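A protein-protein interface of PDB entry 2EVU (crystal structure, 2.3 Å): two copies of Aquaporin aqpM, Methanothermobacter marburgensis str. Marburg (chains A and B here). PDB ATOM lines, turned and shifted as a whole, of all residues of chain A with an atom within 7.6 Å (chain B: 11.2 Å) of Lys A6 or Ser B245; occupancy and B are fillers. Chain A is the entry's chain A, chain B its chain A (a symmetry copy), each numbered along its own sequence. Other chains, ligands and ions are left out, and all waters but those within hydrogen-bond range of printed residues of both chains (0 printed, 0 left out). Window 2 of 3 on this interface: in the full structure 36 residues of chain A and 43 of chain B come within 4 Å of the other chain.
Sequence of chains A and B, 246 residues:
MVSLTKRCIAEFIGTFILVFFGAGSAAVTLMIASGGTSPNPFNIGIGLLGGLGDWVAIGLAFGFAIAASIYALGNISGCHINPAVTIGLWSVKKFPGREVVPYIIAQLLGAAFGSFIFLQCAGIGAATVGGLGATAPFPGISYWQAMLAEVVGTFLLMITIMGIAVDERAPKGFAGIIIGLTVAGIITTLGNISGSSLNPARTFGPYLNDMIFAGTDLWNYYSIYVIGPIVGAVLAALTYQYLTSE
NZ of Lys A6 sits at hydrogen-bond distance from O of Tyr B242 (2.8 Å). OG of Ser B245 is in hydrogen-bond range of NZ of Lys A6, 2.8 Å away.
Of the 16 printed residues of chain B, 6 touch a printed residue of chain A. Of the 16 printed residues of chain A, 6 touch a printed residue of chain B. Among the printed residues, 9 pairs touch across the chains.
Val A2 touches Leu B243. Leu B243 touches Lys A6 (CD2 to O, 3.5 Å). Ile A9 touches Leu B243. Ile A13 touches Thr B239 (CD1 to CG2, 3.9 Å). Ile B159 touches Leu A73 (CD1 to CD2, 3.9 Å). Ile A76 touches Leu B243 (CD1 to CB, 3.8 Å). Thr B244 touches Ile A76 (CG2 to CD1, 3.97 Å).
No position is printed for both chains. Of the 9 pairs that touch across the chains among the printed residues, none has its exchanged pair printed and touching as well.
Lys A6 touches just these residues of chain B: Tyr B242, Leu B243 and Ser B245. Of chain A, only Lys A6 (2.8 Å) comes within 4 Å of Ser B245. No residue of chain B comes within 4 Å of Thr A5. No residue of chain B comes within 4 Å of Cys A8. Of the printed residues of chain A, Leu B243 touches Val A2, Lys A6, Ile A9 and Ile A76. Printed residues of chain B within 4 Å of Ile A76: Leu B243 (3.8 Å) and Thr B244 (3.97 Å). Printed residues of chain B within 4 Å of Val A2: Leu B243 (3.9 Å). Of the printed residues of chain A, Thr B244 touches Ile A76 (3.97 Å). Of the printed residues of chain A, Tyr B242 touches Lys A6. Gln B241 touches none of the printed residues of chain A. The nearest printed residue of chain A that does not touch Leu B243 is Ile A13 (4.1 Å).
NH1 of Arg A7 lies close to O of Val A2 (3.5 Å). The side-chain hydroxyl (OG) of Ser A3 is in hydrogen-bond range of the backbone NH (N) of Lys A6 (3.3 Å). The backbone carbonyl oxygen (O) of Tyr B240 sits at hydrogen-bond distance from the side-chain hydroxyl (OG1) of Thr B244, at 2.7 Å. O of Tyr B242 is in hydrogen-bond range of OG of Ser B245.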
ATOM      1  N   VAL A   2     -28.750  -0.111  -8.765  1.00  0.00           N
ATOM      2  CA  VAL A   2     -28.863   1.341  -8.658  1.00  0.00           C
ATOM      3  C   VAL A   2     -28.929   1.885 -10.082  1.00  0.00           C
ATOM      4  O   VAL A   2     -28.260   1.365 -10.972  1.00  0.00           O
ATOM      5  CB  VAL A   2     -27.647   1.959  -7.928  1.00  0.00           C
ATOM      6  CG1 VAL A   2     -27.687   3.473  -8.023  1.00  0.00           C
ATOM      7  CG2 VAL A   2     -27.653   1.540  -6.469  1.00  0.00           C
ATOM      8  N   SER A   3     -29.737   2.920 -10.298  1.00  0.00           N
ATOM      9  CA  SER A   3     -29.887   3.509 -11.630  1.00  0.00           C
ATOM     10  C   SER A   3     -28.555   4.004 -12.203  1.00  0.00           C
ATOM     11  O   SER A   3     -27.700   4.512 -11.470  1.00  0.00           O
ATOM     12  CB  SER A   3     -30.892   4.667 -11.588  1.00  0.00           C
ATOM     13  OG  SER A   3     -30.372   5.794 -10.899  1.00  0.00           O
ATOM     14  N   LEU A   4     -28.389   3.860 -13.517  1.00  0.00           N
ATOM     15  CA  LEU A   4     -27.165   4.285 -14.188  1.00  0.00           C
ATOM     16  C   LEU A   4     -26.879   5.754 -13.901  1.00  0.00           C
ATOM     17  O   LEU A   4     -25.725   6.182 -13.841  1.00  0.00           O
ATOM     18  CB  LEU A   4     -27.295   4.095 -15.701  1.00  0.00           C
ATOM     19  CG  LEU A   4     -26.048   3.736 -16.526  1.00  0.00           C
ATOM     20  CD1 LEU A   4     -26.298   4.120 -17.982  1.00  0.00           C
ATOM     21  CD2 LEU A   4     -24.815   4.451 -16.007  1.00  0.00           C
ATOM     22  N   THR A   5     -27.939   6.533 -13.726  1.00  0.00           N
ATOM     23  CA  THR A   5     -27.775   7.952 -13.462  1.00  0.00           C
ATOM     24  C   THR A   5     -27.116   8.193 -12.110  1.00  0.00           C
ATOM     25  O   THR A   5     -26.241   9.048 -11.981  1.00  0.00           O
ATOM     26  CB  THR A   5     -29.128   8.695 -13.515  1.00  0.00           C
ATOM     27  OG1 THR A   5     -28.898  10.106 -13.426  1.00  0.00           O
ATOM     28  CG2 THR A   5     -30.018   8.270 -12.362  1.00  0.00           C
ATOM     29  N   LYS A   6     -27.533   7.438 -11.101  1.00  0.00           N
ATOM     30  CA  LYS A   6     -26.957   7.589  -9.773  1.00  0.00           C
ATOM     31  C   LYS A   6     -25.577   6.943  -9.685  1.00  0.00           C
ATOM     32  O   LYS A   6     -24.714   7.409  -8.945  1.00  0.00           O
ATOM     33  CB  LYS A   6     -27.892   7.004  -8.717  1.00  0.00           C
ATOM     34  CG  LYS A   6     -29.058   7.921  -8.383  1.00  0.00           C
ATOM     35  CD  LYS A   6     -29.936   7.326  -7.298  1.00  0.00           C
ATOM     36  CE  LYS A   6     -31.047   8.281  -6.878  1.00  0.00           C
ATOM     37  NZ  LYS A   6     -31.941   7.644  -5.862  1.00  0.00           N
ATOM     38  N   ARG A   7     -25.369   5.877 -10.451  1.00  0.00           N
ATOM     39  CA  ARG A   7     -24.080   5.208 -10.456  1.00  0.00           C
ATOM     40  C   ARG A   7     -23.065   6.099 -11.171  1.00  0.00           C
ATOM     41  O   ARG A   7     -21.864   6.020 -10.918  1.00  0.00           O
ATOM     42  CB  ARG A   7     -24.191   3.850 -11.146  1.00  0.00           C
ATOM     43  CG  ARG A   7     -24.909   2.802 -10.309  1.00  0.00           C
ATOM     44  CD  ARG A   7     -25.527   1.754 -11.215  1.00  0.00           C
ATOM     45  NE  ARG A   7     -24.608   1.381 -12.282  1.00  0.00           N
ATOM     46  CZ  ARG A   7     -24.981   0.913 -13.467  1.00  0.00           C
ATOM     47  NH1 ARG A   7     -26.269   0.752 -13.750  1.00  0.00           N
ATOM     48  NH2 ARG A   7     -24.060   0.624 -14.376  1.00  0.00           N
ATOM     49  N   CYS A   8     -23.559   6.951 -12.066  1.00  0.00           N
ATOM     50  CA  CYS A   8     -22.692   7.874 -12.790  1.00  0.00           C
ATOM     51  C   CYS A   8     -22.336   9.018 -11.851  1.00  0.00           C
ATOM     52  O   CYS A   8     -21.218   9.531 -11.874  1.00  0.00           O
ATOM     53  CB  CYS A   8     -23.392   8.413 -14.044  1.00  0.00           C
ATOM     54  SG  CYS A   8     -23.333   7.283 -15.465  1.00  0.00           S
ATOM     55  N   ILE A   9     -23.288   9.423 -11.021  1.00  0.00           N
ATOM     56  CA  ILE A   9     -23.012  10.480 -10.064  1.00  0.00           C
ATOM     57  C   ILE A   9     -21.933   9.942  -9.113  1.00  0.00           C
ATOM     58  O   ILE A   9     -20.975  10.640  -8.785  1.00  0.00           O
ATOM     59  CB  ILE A   9     -24.272  10.850  -9.270  1.00  0.00           C
ATOM     60  CG1 ILE A   9     -25.306  11.473 -10.220  1.00  0.00           C
ATOM     61  CG2 ILE A   9     -23.915  11.805  -8.133  1.00  0.00           C
ATOM     62  CD1 ILE A   9     -26.617  11.857  -9.551  1.00  0.00           C
ATOM     63  N   ALA A  10     -22.086   8.688  -8.701  1.00  0.00           N
ATOM     64  CA  ALA A  10     -21.130   8.055  -7.809  1.00  0.00           C
ATOM     65  C   ALA A  10     -19.729   8.061  -8.427  1.00  0.00           C
ATOM     66  O   ALA A  10     -18.752   8.454  -7.777  1.00  0.00           O
ATOM     67  CB  ALA A  10     -21.573   6.621  -7.501  1.00  0.00           C
ATOM     68  N   GLU A  11     -19.633   7.622  -9.679  1.00  0.00           N
ATOM     69  CA  GLU A  11     -18.352   7.593 -10.376  1.00  0.00           C
ATOM     70  C   GLU A  11     -17.767   8.996 -10.415  1.00  0.00           C
ATOM     71  O   GLU A  11     -16.550   9.183 -10.334  1.00  0.00           O
ATOM     72  CB  GLU A  11     -18.530   7.076 -11.804  1.00  0.00           C
ATOM     73  CG  GLU A  11     -18.836   5.594 -11.901  1.00  0.00           C
ATOM     74  CD  GLU A  11     -17.714   4.722 -11.349  1.00  0.00           C
ATOM     75  OE1 GLU A  11     -16.558   4.859 -11.813  1.00  0.00           O
ATOM     76  OE2 GLU A  11     -17.993   3.892 -10.457  1.00  0.00           O
ATOM     77  N   PHE A  12     -18.645   9.984 -10.544  1.00  0.00           N
ATOM     78  CA  PHE A  12     -18.224  11.374 -10.594  1.00  0.00           C
ATOM     79  C   PHE A  12     -17.543  11.731  -9.274  1.00  0.00           C
ATOM     80  O   PHE A  12     -16.412  12.227  -9.256  1.00  0.00           O
ATOM     81  CB  PHE A  12     -19.444  12.275 -10.845  1.00  0.00           C
ATOM     82  CG  PHE A  12     -19.139  13.749 -10.795  1.00  0.00           C
ATOM     83  CD1 PHE A  12     -19.190  14.441  -9.590  1.00  0.00           C
ATOM     84  CD2 PHE A  12     -18.776  14.434 -11.946  1.00  0.00           C
ATOM     85  CE1 PHE A  12     -18.880  15.799  -9.531  1.00  0.00           C
ATOM     86  CE2 PHE A  12     -18.464  15.786 -11.901  1.00  0.00           C
ATOM     87  CZ  PHE A  12     -18.515  16.473 -10.690  1.00  0.00           C
ATOM     88  N   ILE A  13     -18.240  11.461  -8.178  1.00  0.00           N
ATOM     89  CA  ILE A  13     -17.745  11.728  -6.834  1.00  0.00           C
ATOM     90  C   ILE A  13     -16.442  10.970  -6.543  1.00  0.00           C
ATOM     91  O   ILE A  13     -15.481  11.546  -6.032  1.00  0.00           O
ATOM     92  CB  ILE A  13     -18.818  11.335  -5.805  1.00  0.00           C
ATOM     93  CG1 ILE A  13     -19.998  12.302  -5.929  1.00  0.00           C
ATOM     94  CG2 ILE A  13     -18.234  11.326  -4.403  1.00  0.00           C
ATOM     95  CD1 ILE A  13     -21.213  11.938  -5.095  1.00  0.00           C
ATOM     96  N   LEU A  73     -18.599   3.979  -2.157  1.00  0.00           N
ATOM     97  CA  LEU A  73     -19.345   3.918  -3.408  1.00  0.00           C
ATOM     98  C   LEU A  73     -19.336   2.580  -4.131  1.00  0.00           C
ATOM     99  O   LEU A  73     -19.990   2.425  -5.160  1.00  0.00           O
ATOM    100  CB  LEU A  73     -18.801   4.993  -4.345  1.00  0.00           C
ATOM    101  CG  LEU A  73     -18.600   6.341  -3.649  1.00  0.00           C
ATOM    102  CD1 LEU A  73     -17.769   7.247  -4.523  1.00  0.00           C
ATOM    103  CD2 LEU A  73     -19.950   6.958  -3.326  1.00  0.00           C
ATOM    104  N   ILE A  76     -22.662   1.015  -4.733  1.00  0.00           N
ATOM    105  CA  ILE A  76     -23.479   1.857  -5.580  1.00  0.00           C
ATOM    106  C   ILE A  76     -23.154   1.645  -7.049  1.00  0.00           C
ATOM    107  O   ILE A  76     -23.989   1.152  -7.796  1.00  0.00           O
ATOM    108  CB  ILE A  76     -23.297   3.342  -5.217  1.00  0.00           C
ATOM    109  CG1 ILE A  76     -23.717   3.569  -3.759  1.00  0.00           C
ATOM    110  CG2 ILE A  76     -24.119   4.217  -6.161  1.00  0.00           C
ATOM    111  CD1 ILE A  76     -23.448   4.966  -3.248  1.00  0.00           C
ATOM    112  N   SER A  77     -21.938   1.992  -7.462  1.00  0.00           N
ATOM    113  CA  SER A  77     -21.560   1.846  -8.866  1.00  0.00           C
ATOM    114  C   SER A  77     -20.434   0.861  -9.181  1.00  0.00           C
ATOM    115  O   SER A  77     -20.147   0.613 -10.356  1.00  0.00           O
ATOM    116  CB  SER A  77     -21.166   3.208  -9.438  1.00  0.00           C
ATOM    117  OG  SER A  77     -19.922   3.643  -8.908  1.00  0.00           O
ATOM    118  N   TYR A 103     -19.869   5.953 -17.913  1.00  0.00           N
ATOM    119  CA  TYR A 103     -18.956   5.936 -16.761  1.00  0.00           C
ATOM    120  C   TYR A 103     -17.715   6.774 -17.049  1.00  0.00           C
ATOM    121  O   TYR A 103     -17.358   7.667 -16.279  1.00  0.00           O
ATOM    122  CB  TYR A 103     -18.506   4.506 -16.421  1.00  0.00           C
ATOM    123  CG  TYR A 103     -19.324   3.814 -15.345  1.00  0.00           C
ATOM    124  CD1 TYR A 103     -18.713   2.945 -14.435  1.00  0.00           C
ATOM    125  CD2 TYR A 103     -20.704   4.003 -15.248  1.00  0.00           C
ATOM    126  CE1 TYR A 103     -19.454   2.281 -13.457  1.00  0.00           C
ATOM    127  CE2 TYR A 103     -21.456   3.344 -14.273  1.00  0.00           C
ATOM    128  CZ  TYR A 103     -20.823   2.485 -13.381  1.00  0.00           C
ATOM    129  OH  TYR A 103     -21.560   1.833 -12.412  1.00  0.00           O
ATOM    130  N   VAL B  92     -29.539  12.080   9.518  1.00  0.00           N
ATOM    131  CA  VAL B  92     -30.176  11.062   8.694  1.00  0.00           C
ATOM    132  C   VAL B  92     -30.834   9.976   9.541  1.00  0.00           C
ATOM    133  O   VAL B  92     -30.892   8.806   9.152  1.00  0.00           O
ATOM    134  CB  VAL B  92     -29.173  10.442   7.697  1.00  0.00           C
ATOM    135  CG1 VAL B  92     -28.733  11.507   6.698  1.00  0.00           C
ATOM    136  CG2 VAL B  92     -27.963   9.876   8.440  1.00  0.00           C
ATOM    137  N   ILE B 159     -18.871  10.239   4.237  1.00  0.00           N
ATOM    138  CA  ILE B 159     -19.437   9.335   3.261  1.00  0.00           C
ATOM    139  C   ILE B 159     -18.782   7.952   3.400  1.00  0.00           C
ATOM    140  O   ILE B 159     -19.402   6.928   3.105  1.00  0.00           O
ATOM    141  CB  ILE B 159     -19.304   9.911   1.827  1.00  0.00           C
ATOM    142  CG1 ILE B 159     -20.198   9.113   0.876  1.00  0.00           C
ATOM    143  CG2 ILE B 159     -17.862   9.893   1.371  1.00  0.00           C
ATOM    144  CD1 ILE B 159     -20.290   9.694  -0.512  1.00  0.00           C
ATOM    145  N   MET B 162     -20.495   6.450   6.349  1.00  0.00           N
ATOM    146  CA  MET B 162     -21.826   6.041   5.934  1.00  0.00           C
ATOM    147  C   MET B 162     -21.742   4.703   5.225  1.00  0.00           C
ATOM    148  O   MET B 162     -22.513   3.785   5.511  1.00  0.00           O
ATOM    149  CB  MET B 162     -22.433   7.074   4.980  1.00  0.00           C
ATOM    150  CG  MET B 162     -22.850   8.380   5.636  1.00  0.00           C
ATOM    151  SD  MET B 162     -24.182   8.134   6.826  1.00  0.00           S
ATOM    152  CE  MET B 162     -25.561   7.675   5.689  1.00  0.00           C
ATOM    153  N   ASP B 167     -24.114   1.670   6.672  1.00  0.00           N
ATOM    154  CA  ASP B 167     -24.789   0.782   5.746  1.00  0.00           C
ATOM    155  C   ASP B 167     -24.710  -0.642   6.260  1.00  0.00           C
ATOM    156  O   ASP B 167     -23.643  -1.134   6.614  1.00  0.00           O
ATOM    157  CB  ASP B 167     -24.165   0.860   4.357  1.00  0.00           C
ATOM    158  CG  ASP B 167     -25.030   0.204   3.296  1.00  0.00           C
ATOM    159  OD1 ASP B 167     -25.482   0.920   2.381  1.00  0.00           O
ATOM    160  OD2 ASP B 167     -25.266  -1.020   3.376  1.00  0.00           O
ATOM    161  N   GLU B 168     -25.862  -1.293   6.286  1.00  0.00           N
ATOM    162  CA  GLU B 168     -26.014  -2.663   6.760  1.00  0.00           C
ATOM    163  C   GLU B 168     -25.240  -3.699   5.946  1.00  0.00           C
ATOM    164  O   GLU B 168     -25.031  -4.816   6.401  1.00  0.00           O
ATOM    165  CB  GLU B 168     -27.504  -3.019   6.762  1.00  0.00           C
ATOM    166  CG  GLU B 168     -28.383  -1.960   7.441  1.00  0.00           C
ATOM    167  CD  GLU B 168     -28.445  -0.614   6.689  1.00  0.00           C
ATOM    168  OE1 GLU B 168     -28.843   0.394   7.321  1.00  0.00           O
ATOM    169  OE2 GLU B 168     -28.115  -0.561   5.478  1.00  0.00           O
ATOM    170  N   ARG B 169     -24.815  -3.330   4.746  1.00  0.00           N
ATOM    171  CA  ARG B 169     -24.079  -4.259   3.894  1.00  0.00           C
ATOM    172  C   ARG B 169     -22.559  -4.175   4.057  1.00  0.00           C
ATOM    173  O   ARG B 169     -21.818  -4.941   3.440  1.00  0.00           O
ATOM    174  CB  ARG B 169     -24.450  -4.013   2.433  1.00  0.00           C
ATOM    175  CG  ARG B 169     -25.918  -4.265   2.124  1.00  0.00           C
ATOM    176  CD  ARG B 169     -26.289  -3.733   0.747  1.00  0.00           C
ATOM    177  NE  ARG B 169     -26.142  -2.283   0.679  1.00  0.00           N
ATOM    178  CZ  ARG B 169     -26.142  -1.582  -0.452  1.00  0.00           C
ATOM    179  NH1 ARG B 169     -26.285  -2.201  -1.617  1.00  0.00           N
ATOM    180  NH2 ARG B 169     -25.982  -0.263  -0.419  1.00  0.00           N
ATOM    181  N   ALA B 236     -22.535  14.921   3.112  1.00  0.00           N
ATOM    182  CA  ALA B 236     -22.151  13.550   2.806  1.00  0.00           C
ATOM    183  C   ALA B 236     -23.243  12.558   3.183  1.00  0.00           C
ATOM    184  O   ALA B 236     -23.570  11.655   2.415  1.00  0.00           O
ATOM    185  CB  ALA B 236     -20.852  13.201   3.540  1.00  0.00           C
ATOM    186  N   ALA B 237     -23.805  12.731   4.372  1.00  0.00           N
ATOM    187  CA  ALA B 237     -24.848  11.844   4.864  1.00  0.00           C
ATOM    188  C   ALA B 237     -26.046  11.841   3.933  1.00  0.00           C
ATOM    189  O   ALA B 237     -26.543  10.776   3.545  1.00  0.00           O
ATOM    190  CB  ALA B 237     -25.267  12.264   6.266  1.00  0.00           C
ATOM    191  N   LEU B 238     -26.505  13.038   3.571  1.00  0.00           N
ATOM    192  CA  LEU B 238     -27.647  13.182   2.668  1.00  0.00           C
ATOM    193  C   LEU B 238     -27.330  12.642   1.282  1.00  0.00           C
ATOM    194  O   LEU B 238     -28.131  11.924   0.689  1.00  0.00           O
ATOM    195  CB  LEU B 238     -28.057  14.654   2.572  1.00  0.00           C
ATOM    196  CG  LEU B 238     -29.095  15.181   3.576  1.00  0.00           C
ATOM    197  CD1 LEU B 238     -28.964  14.490   4.927  1.00  0.00           C
ATOM    198  CD2 LEU B 238     -28.920  16.678   3.711  1.00  0.00           C
ATOM    199  N   THR B 239     -26.155  12.986   0.769  1.00  0.00           N
ATOM    200  CA  THR B 239     -25.748  12.526  -0.558  1.00  0.00           C
ATOM    201  C   THR B 239     -25.797  11.002  -0.630  1.00  0.00           C
ATOM    202  O   THR B 239     -26.289  10.424  -1.605  1.00  0.00           O
ATOM    203  CB  THR B 239     -24.318  12.986  -0.885  1.00  0.00           C
ATOM    204  OG1 THR B 239     -24.254  14.412  -0.814  1.00  0.00           O
ATOM    205  CG2 THR B 239     -23.907  12.528  -2.279  1.00  0.00           C
ATOM    206  N   TYR B 240     -25.284  10.361   0.417  1.00  0.00           N
ATOM    207  CA  TYR B 240     -25.262   8.910   0.481  1.00  0.00           C
ATOM    208  C   TYR B 240     -26.674   8.351   0.620  1.00  0.00           C
ATOM    209  O   TYR B 240     -26.966   7.259   0.139  1.00  0.00           O
ATOM    210  CB  TYR B 240     -24.380   8.452   1.650  1.00  0.00           C
ATOM    211  CG  TYR B 240     -24.206   6.951   1.713  1.00  0.00           C
ATOM    212  CD1 TYR B 240     -25.122   6.155   2.400  1.00  0.00           C
ATOM    213  CD2 TYR B 240     -23.152   6.323   1.047  1.00  0.00           C
ATOM    214  CE1 TYR B 240     -24.998   4.772   2.423  1.00  0.00           C
ATOM    215  CE2 TYR B 240     -23.018   4.940   1.063  1.00  0.00           C
ATOM    216  CZ  TYR B 240     -23.947   4.170   1.756  1.00  0.00           C
ATOM    217  OH  TYR B 240     -23.833   2.800   1.786  1.00  0.00           O
ATOM    218  N   GLN B 241     -27.545   9.100   1.287  1.00  0.00           N
ATOM    219  CA  GLN B 241     -28.933   8.684   1.462  1.00  0.00           C
ATOM    220  C   GLN B 241     -29.638   8.702   0.108  1.00  0.00           C
ATOM    221  O   GLN B 241     -30.451   7.830  -0.199  1.00  0.00           O
ATOM    222  CB  GLN B 241     -29.652   9.631   2.421  1.00  0.00           C
ATOM    223  CG  GLN B 241     -31.110   9.275   2.669  1.00  0.00           C
ATOM    224  CD  GLN B 241     -31.744  10.109   3.776  1.00  0.00           C
ATOM    225  OE1 GLN B 241     -31.908  11.326   3.641  1.00  0.00           O
ATOM    226  NE2 GLN B 241     -32.099   9.455   4.881  1.00  0.00           N
ATOM    227  N   TYR B 242     -29.309   9.704  -0.700  1.00  0.00           N
ATOM    228  CA  TYR B 242     -29.885   9.864  -2.029  1.00  0.00           C
ATOM    229  C   TYR B 242     -29.389   8.799  -3.007  1.00  0.00           C
ATOM    230  O   TYR B 242     -30.177   8.183  -3.727  1.00  0.00           O
ATOM    231  CB  TYR B 242     -29.536  11.255  -2.565  1.00  0.00           C
ATOM    232  CG  TYR B 242     -29.820  11.452  -4.037  1.00  0.00           C
ATOM    233  CD1 TYR B 242     -31.123  11.630  -4.502  1.00  0.00           C
ATOM    234  CD2 TYR B 242     -28.783  11.443  -4.968  1.00  0.00           C
ATOM    235  CE1 TYR B 242     -31.386  11.797  -5.859  1.00  0.00           C
ATOM    236  CE2 TYR B 242     -29.031  11.608  -6.330  1.00  0.00           C
ATOM    237  CZ  TYR B 242     -30.336  11.785  -6.770  1.00  0.00           C
ATOM    238  OH  TYR B 242     -30.583  11.950  -8.117  1.00  0.00           O
ATOM    239  N   LEU B 243     -28.078   8.587  -3.032  1.00  0.00           N
ATOM    240  CA  LEU B 243     -27.486   7.617  -3.941  1.00  0.00           C
ATOM    241  C   LEU B 243     -27.920   6.182  -3.679  1.00  0.00           C
ATOM    242  O   LEU B 243     -27.949   5.360  -4.598  1.00  0.00           O
ATOM    243  CB  LEU B 243     -25.960   7.709  -3.889  1.00  0.00           C
ATOM    244  CG  LEU B 243     -25.319   8.968  -4.480  1.00  0.00           C
ATOM    245  CD1 LEU B 243     -23.819   8.953  -4.210  1.00  0.00           C
ATOM    246  CD2 LEU B 243     -25.591   9.029  -5.975  1.00  0.00           C
ATOM    247  N   THR B 244     -28.249   5.871  -2.430  1.00  0.00           N
ATOM    248  CA  THR B 244     -28.671   4.521  -2.103  1.00  0.00           C
ATOM    249  C   THR B 244     -30.188   4.436  -2.000  1.00  0.00           C
ATOM    250  O   THR B 244     -30.736   3.398  -1.635  1.00  0.00           O
ATOM    251  CB  THR B 244     -28.024   4.031  -0.784  1.00  0.00           C
ATOM    252  OG1 THR B 244     -28.349   4.931   0.282  1.00  0.00           O
ATOM    253  CG2 THR B 244     -26.510   3.955  -0.930  1.00  0.00           C
ATOM    254  N   SER B 245     -30.864   5.532  -2.332  1.00  0.00           N
ATOM    255  CA  SER B 245     -32.327   5.571  -2.285  1.00  0.00           C
ATOM    256  C   SER B 245     -32.914   5.116  -3.615  1.00  0.00           C
ATOM    257  O   SER B 245     -34.003   4.544  -3.647  1.00  0.00           O
ATOM    258  CB  SER B 245     -32.829   6.984  -1.993  1.00  0.00           C
ATOM    259  OG  SER B 245     -32.793   7.774  -3.172  1.00  0.00           O
